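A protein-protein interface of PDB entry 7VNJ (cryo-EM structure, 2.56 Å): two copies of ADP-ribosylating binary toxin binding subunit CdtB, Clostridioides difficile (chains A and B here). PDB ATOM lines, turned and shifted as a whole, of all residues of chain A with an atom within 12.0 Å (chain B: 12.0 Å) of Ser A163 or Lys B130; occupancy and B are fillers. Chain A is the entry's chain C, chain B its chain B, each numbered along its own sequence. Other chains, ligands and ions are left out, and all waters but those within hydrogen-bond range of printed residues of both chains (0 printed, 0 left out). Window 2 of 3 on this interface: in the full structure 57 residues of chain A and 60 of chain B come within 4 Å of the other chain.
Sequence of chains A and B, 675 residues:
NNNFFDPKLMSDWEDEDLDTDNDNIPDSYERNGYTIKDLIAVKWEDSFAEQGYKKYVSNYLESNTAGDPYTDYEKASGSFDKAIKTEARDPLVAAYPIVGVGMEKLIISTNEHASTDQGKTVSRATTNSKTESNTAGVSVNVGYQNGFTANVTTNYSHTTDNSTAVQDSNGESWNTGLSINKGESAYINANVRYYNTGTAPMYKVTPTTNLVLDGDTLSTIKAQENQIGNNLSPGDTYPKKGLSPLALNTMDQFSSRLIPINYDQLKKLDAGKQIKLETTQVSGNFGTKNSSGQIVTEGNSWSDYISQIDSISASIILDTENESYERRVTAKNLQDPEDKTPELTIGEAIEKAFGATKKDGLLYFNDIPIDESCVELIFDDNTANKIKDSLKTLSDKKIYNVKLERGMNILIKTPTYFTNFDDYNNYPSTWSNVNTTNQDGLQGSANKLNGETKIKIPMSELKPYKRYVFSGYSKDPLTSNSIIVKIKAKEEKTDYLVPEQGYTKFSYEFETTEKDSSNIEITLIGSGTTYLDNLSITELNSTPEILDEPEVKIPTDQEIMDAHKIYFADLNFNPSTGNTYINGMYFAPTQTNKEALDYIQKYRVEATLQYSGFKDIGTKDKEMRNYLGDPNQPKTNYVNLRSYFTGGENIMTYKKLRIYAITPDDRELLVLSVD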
ATOM      1  N   ALA A 125       3.767 -20.003   4.931  1.00  0.00           N
ATOM      2  CA  ALA A 125       4.993 -20.783   5.010  1.00  0.00           C
ATOM      3  C   ALA A 125       4.911 -21.782   6.156  1.00  0.00           C
ATOM      4  O   ALA A 125       4.173 -21.592   7.126  1.00  0.00           O
ATOM      5  CB  ALA A 125       6.222 -19.883   5.191  1.00  0.00           C
ATOM      6  N   THR A 126       5.684 -22.860   6.026  1.00  0.00           N
ATOM      7  CA  THR A 126       5.759 -23.908   7.036  1.00  0.00           C
ATOM      8  C   THR A 126       7.203 -24.371   7.149  1.00  0.00           C
ATOM      9  O   THR A 126       7.853 -24.626   6.131  1.00  0.00           O
ATOM     10  CB  THR A 126       4.848 -25.089   6.680  1.00  0.00           C
ATOM     11  OG1 THR A 126       3.483 -24.655   6.667  1.00  0.00           O
ATOM     12  CG2 THR A 126       5.005 -26.214   7.691  1.00  0.00           C
ATOM     13  N   THR A 127       7.702 -24.485   8.378  1.00  0.00           N
ATOM     14  CA  THR A 127       9.093 -24.839   8.626  1.00  0.00           C
ATOM     15  C   THR A 127       9.174 -26.020   9.583  1.00  0.00           C
ATOM     16  O   THR A 127       8.456 -26.070  10.584  1.00  0.00           O
ATOM     17  CB  THR A 127       9.873 -23.650   9.207  1.00  0.00           C
ATOM     18  OG1 THR A 127       9.575 -22.468   8.455  1.00  0.00           O
ATOM     19  CG2 THR A 127      11.370 -23.914   9.157  1.00  0.00           C
ATOM     20  N   ASN A 128      10.056 -26.967   9.265  1.00  0.00           N
ATOM     21  CA  ASN A 128      10.336 -28.116  10.120  1.00  0.00           C
ATOM     22  C   ASN A 128      11.832 -28.151  10.388  1.00  0.00           C
ATOM     23  O   ASN A 128      12.633 -28.107   9.449  1.00  0.00           O
ATOM     24  CB  ASN A 128       9.879 -29.424   9.466  1.00  0.00           C
ATOM     25  CG  ASN A 128       8.375 -29.605   9.506  1.00  0.00           C
ATOM     26  OD1 ASN A 128       7.617 -28.639   9.433  1.00  0.00           O
ATOM     27  ND2 ASN A 128       7.935 -30.851   9.624  1.00  0.00           N
ATOM     28  N   SER A 129      12.209 -28.236  11.661  1.00  0.00           N
ATOM     29  CA  SER A 129      13.607 -28.194  12.063  1.00  0.00           C
ATOM     30  C   SER A 129      13.992 -29.471  12.798  1.00  0.00           C
ATOM     31  O   SER A 129      13.139 -30.221  13.280  1.00  0.00           O
ATOM     32  CB  SER A 129      13.893 -26.976  12.949  1.00  0.00           C
ATOM     33  OG  SER A 129      13.608 -25.769  12.264  1.00  0.00           O
ATOM     34  N   LYS A 130      15.301 -29.707  12.878  1.00  0.00           N
ATOM     35  CA  LYS A 130      15.840 -30.876  13.570  1.00  0.00           C
ATOM     36  C   LYS A 130      17.297 -30.606  13.901  1.00  0.00           C
ATOM     37  O   LYS A 130      18.116 -30.441  12.993  1.00  0.00           O
ATOM     38  CB  LYS A 130      15.703 -32.132  12.709  1.00  0.00           C
ATOM     39  CG  LYS A 130      16.403 -33.354  13.278  1.00  0.00           C
ATOM     40  CD  LYS A 130      16.075 -34.599  12.468  1.00  0.00           C
ATOM     41  CE  LYS A 130      16.729 -35.835  13.063  1.00  0.00           C
ATOM     42  NZ  LYS A 130      18.208 -35.689  13.150  1.00  0.00           N
ATOM     43  N   SER A 163      11.469 -28.664  15.994  1.00  0.00           N
ATOM     44  CA  SER A 163      10.731 -27.415  15.908  1.00  0.00           C
ATOM     45  C   SER A 163       9.754 -27.452  14.742  1.00  0.00           C
ATOM     46  O   SER A 163       9.938 -28.199  13.777  1.00  0.00           O
ATOM     47  CB  SER A 163      11.679 -26.220  15.748  1.00  0.00           C
ATOM     48  OG  SER A 163      12.342 -25.927  16.966  1.00  0.00           O
ATOM     49  N   THR A 164       8.708 -26.639  14.851  1.00  0.00           N
ATOM     50  CA  THR A 164       7.754 -26.448  13.772  1.00  0.00           C
ATOM     51  C   THR A 164       7.261 -25.010  13.822  1.00  0.00           C
ATOM     52  O   THR A 164       7.284 -24.369  14.876  1.00  0.00           O
ATOM     53  CB  THR A 164       6.575 -27.427  13.863  1.00  0.00           C
ATOM     54  OG1 THR A 164       5.745 -27.290  12.704  1.00  0.00           O
ATOM     55  CG2 THR A 164       5.746 -27.156  15.108  1.00  0.00           C
ATOM     56  N   ALA A 165       6.828 -24.502  12.671  1.00  0.00           N
ATOM     57  CA  ALA A 165       6.378 -23.122  12.586  1.00  0.00           C
ATOM     58  C   ALA A 165       5.453 -22.967  11.390  1.00  0.00           C
ATOM     59  O   ALA A 165       5.668 -23.593  10.349  1.00  0.00           O
ATOM     60  CB  ALA A 165       7.561 -22.154  12.472  1.00  0.00           C
ATOM     61  N   VAL A 166       4.428 -22.137  11.551  1.00  0.00           N
ATOM     62  CA  VAL A 166       3.501 -21.800  10.476  1.00  0.00           C
ATOM     63  C   VAL A 166       3.382 -20.285  10.433  1.00  0.00           C
ATOM     64  O   VAL A 166       3.019 -19.659  11.437  1.00  0.00           O
ATOM     65  CB  VAL A 166       2.122 -22.450  10.674  1.00  0.00           C
ATOM     66  CG1 VAL A 166       1.083 -21.767   9.798  1.00  0.00           C
ATOM     67  CG2 VAL A 166       2.192 -23.936  10.370  1.00  0.00           C
ATOM     68  N   GLN A 167       3.682 -19.697   9.279  1.00  0.00           N
ATOM     69  CA  GLN A 167       3.700 -18.251   9.112  1.00  0.00           C
ATOM     70  C   GLN A 167       2.663 -17.847   8.075  1.00  0.00           C
ATOM     71  O   GLN A 167       2.572 -18.464   7.010  1.00  0.00           O
ATOM     72  CB  GLN A 167       5.090 -17.764   8.698  1.00  0.00           C
ATOM     73  CG  GLN A 167       5.200 -16.257   8.552  1.00  0.00           C
ATOM     74  CD  GLN A 167       6.623 -15.800   8.307  1.00  0.00           C
ATOM     75  OE1 GLN A 167       7.477 -16.585   7.897  1.00  0.00           O
ATOM     76  NE2 GLN A 167       6.885 -14.523   8.558  1.00  0.00           N
ATOM     77  N   THR B 126       2.454 -13.222  10.790  1.00  0.00           N
ATOM     78  CA  THR B 126       2.131 -13.884  12.047  1.00  0.00           C
ATOM     79  C   THR B 126       2.768 -15.265  12.041  1.00  0.00           C
ATOM     80  O   THR B 126       2.625 -16.005  11.064  1.00  0.00           O
ATOM     81  CB  THR B 126       0.616 -13.994  12.245  1.00  0.00           C
ATOM     82  OG1 THR B 126       0.051 -12.683  12.366  1.00  0.00           O
ATOM     83  CG2 THR B 126       0.295 -14.792  13.500  1.00  0.00           C
ATOM     84  N   THR B 127       3.463 -15.611  13.124  1.00  0.00           N
ATOM     85  CA  THR B 127       4.183 -16.873  13.225  1.00  0.00           C
ATOM     86  C   THR B 127       3.795 -17.587  14.511  1.00  0.00           C
ATOM     87  O   THR B 127       3.571 -16.948  15.541  1.00  0.00           O
ATOM     88  CB  THR B 127       5.702 -16.650  13.198  1.00  0.00           C
ATOM     89  OG1 THR B 127       6.033 -15.728  12.153  1.00  0.00           O
ATOM     90  CG2 THR B 127       6.434 -17.961  12.955  1.00  0.00           C
ATOM     91  N   ASN B 128       3.723 -18.917  14.446  1.00  0.00           N
ATOM     92  CA  ASN B 128       3.424 -19.766  15.600  1.00  0.00           C
ATOM     93  C   ASN B 128       4.484 -20.862  15.658  1.00  0.00           C
ATOM     94  O   ASN B 128       4.391 -21.857  14.935  1.00  0.00           O
ATOM     95  CB  ASN B 128       2.022 -20.361  15.505  1.00  0.00           C
ATOM     96  CG  ASN B 128       0.930 -19.331  15.723  1.00  0.00           C
ATOM     97  OD1 ASN B 128       1.199 -18.188  16.087  1.00  0.00           O
ATOM     98  ND2 ASN B 128      -0.313 -19.735  15.499  1.00  0.00           N
ATOM     99  N   SER B 129       5.480 -20.687  16.521  1.00  0.00           N
ATOM    100  CA  SER B 129       6.595 -21.619  16.630  1.00  0.00           C
ATOM    101  C   SER B 129       6.413 -22.522  17.843  1.00  0.00           C
ATOM    102  O   SER B 129       6.236 -22.037  18.965  1.00  0.00           O
ATOM    103  CB  SER B 129       7.924 -20.869  16.730  1.00  0.00           C
ATOM    104  OG  SER B 129       8.397 -20.494  15.449  1.00  0.00           O
ATOM    105  N   LYS B 130       6.461 -23.833  17.612  1.00  0.00           N
ATOM    106  CA  LYS B 130       6.366 -24.833  18.667  1.00  0.00           C
ATOM    107  C   LYS B 130       7.575 -25.750  18.581  1.00  0.00           C
ATOM    108  O   LYS B 130       7.917 -26.227  17.495  1.00  0.00           O
ATOM    109  CB  LYS B 130       5.070 -25.641  18.549  1.00  0.00           C
ATOM    110  CG  LYS B 130       4.982 -26.824  19.497  1.00  0.00           C
ATOM    111  CD  LYS B 130       3.663 -27.562  19.330  1.00  0.00           C
ATOM    112  CE  LYS B 130       3.516 -28.680  20.349  1.00  0.00           C
ATOM    113  NZ  LYS B 130       4.501 -29.774  20.129  1.00  0.00           N
ATOM    114  N   SER B 163       5.632 -20.155  21.040  1.00  0.00           N
ATOM    115  CA  SER B 163       6.033 -18.812  20.658  1.00  0.00           C
ATOM    116  C   SER B 163       5.052 -18.241  19.644  1.00  0.00           C
ATOM    117  O   SER B 163       4.338 -18.979  18.960  1.00  0.00           O
ATOM    118  CB  SER B 163       7.449 -18.800  20.072  1.00  0.00           C
ATOM    119  OG  SER B 163       8.392 -19.292  21.007  1.00  0.00           O
ATOM    120  N   THR B 164       5.023 -16.914  19.563  1.00  0.00           N
ATOM    121  CA  THR B 164       4.197 -16.216  18.593  1.00  0.00           C
ATOM    122  C   THR B 164       4.852 -14.881  18.274  1.00  0.00           C
ATOM    123  O   THR B 164       5.679 -14.377  19.039  1.00  0.00           O
ATOM    124  CB  THR B 164       2.766 -16.008  19.108  1.00  0.00           C
ATOM    125  OG1 THR B 164       1.970 -15.399  18.084  1.00  0.00           O
ATOM    126  CG2 THR B 164       2.767 -15.115  20.337  1.00  0.00           C
ATOM    127  N   ALA B 165       4.481 -14.315  17.129  1.00  0.00           N
ATOM    128  CA  ALA B 165       5.053 -13.047  16.704  1.00  0.00           C
ATOM    129  C   ALA B 165       4.099 -12.364  15.738  1.00  0.00           C
ATOM    130  O   ALA B 165       3.342 -13.023  15.022  1.00  0.00           O
ATOM    131  CB  ALA B 165       6.427 -13.240  16.052  1.00  0.00           C
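O of Lys B130 sits at hydrogen-bond distance from N of Thr A164 (2.8 Å). N of Asn B128 is in hydrogen-bond range of O of Val A166 (3.2 Å).
N of Thr A127 is in hydrogen-bond range of O of Ala A165 (3.0 Å). OG1 of Thr B164 lies close to O of Thr B127 (3.4 Å). The backbone carbonyl oxygen (O) of Gln A167 lies within hydrogen-bond range of the backbone NH (N) of Ala A125, at 2.8 Å. The backbone NH of Ser B163 sits at hydrogen-bond distance from the backbone carbonyl oxygen of Ser B129, 2.9 Å away. The backbone NH (N) of Ala B165 lies within hydrogen-bond range of the backbone carbonyl oxygen (O) of Thr B127 (3.2 Å). The backbone carbonyl oxygen of Ser A163 is in hydrogen-bond range of the backbone NH of Ser A129 (3.1 Å).
Ser A163 touches Lys B130. Asn B128 touches Thr A164 (O to O, 3.8 Å). O of Thr A164 touches CA of Ser B129, 3.3 Å away. Ala A165 touches Asn B128. CB of Ala A165 touches OG of Ser B129, 3.5 Å away. Thr B126 touches Val A166. Val A166 touches Thr B127 (O to CA, 3.5 Å). Thr B126 touches Gln A167. OG1 of Thr B127 touches CG of Gln A167, at 3.7 Å.
Ala A125 touches none of the printed residues of chain B. Thr A127 touches none of the printed residues of chain B. Printed residues of chain B within 4 Å of Ser A163: Lys B130 (3.4 Å). Of the printed residues of chain B, Val A166 touches Thr B126, Thr B127 and Asn B128. Of the printed residues of chain B, Gln A167 touches Thr B126 and Thr B127. Of the printed residues of chain A, Thr B126 touches Val A166 (3.7 Å) and Gln A167 (3.2 Å). Of the printed residues of chain A, Thr B127 touches Val A166 (3.5 Å) and Gln A167 (3.7 Å). Printed residues of chain A within 4 Å of Asn B128: Thr A164 (3.8 Å), Ala A165 (3.3 Å) and Val A166 (3.2 Å). Lys B130 touches just these residues of chain A: Ser A163 (3.4 Å) and Thr A164 (2.8 Å). The nearest residue of chain B that does not touch Ser A163 is Ser B129 (6.6 Å).
Of the 11 printed residues of chain A, 5 touch a printed residue of chain B. Hydrophobic or aromatic side chains of chain A within 4 Å of the printed part of chain B: Ala A165. Among the printed residues, no Asp or Glu carboxylate lies within 4 Å of a Lys or Arg side-chain nitrogen of the other chain.
Ser A163 touches Lys B130, but with the chains exchanged Lys A130 does not touch Ser B163 (14.9 Å). Thr A164 touches Asn B128, but with the chains exchanged Asn A128 does not touch Thr B164 (15.2 Å). Thr A164 touches Ser B129, but with the chains exchanged Ser A129 does not touch Thr B164 (14.3 Å). Thr A164 touches Lys B130, but with the chains exchanged Lys A130 does not touch Thr B164 (17.7 Å).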
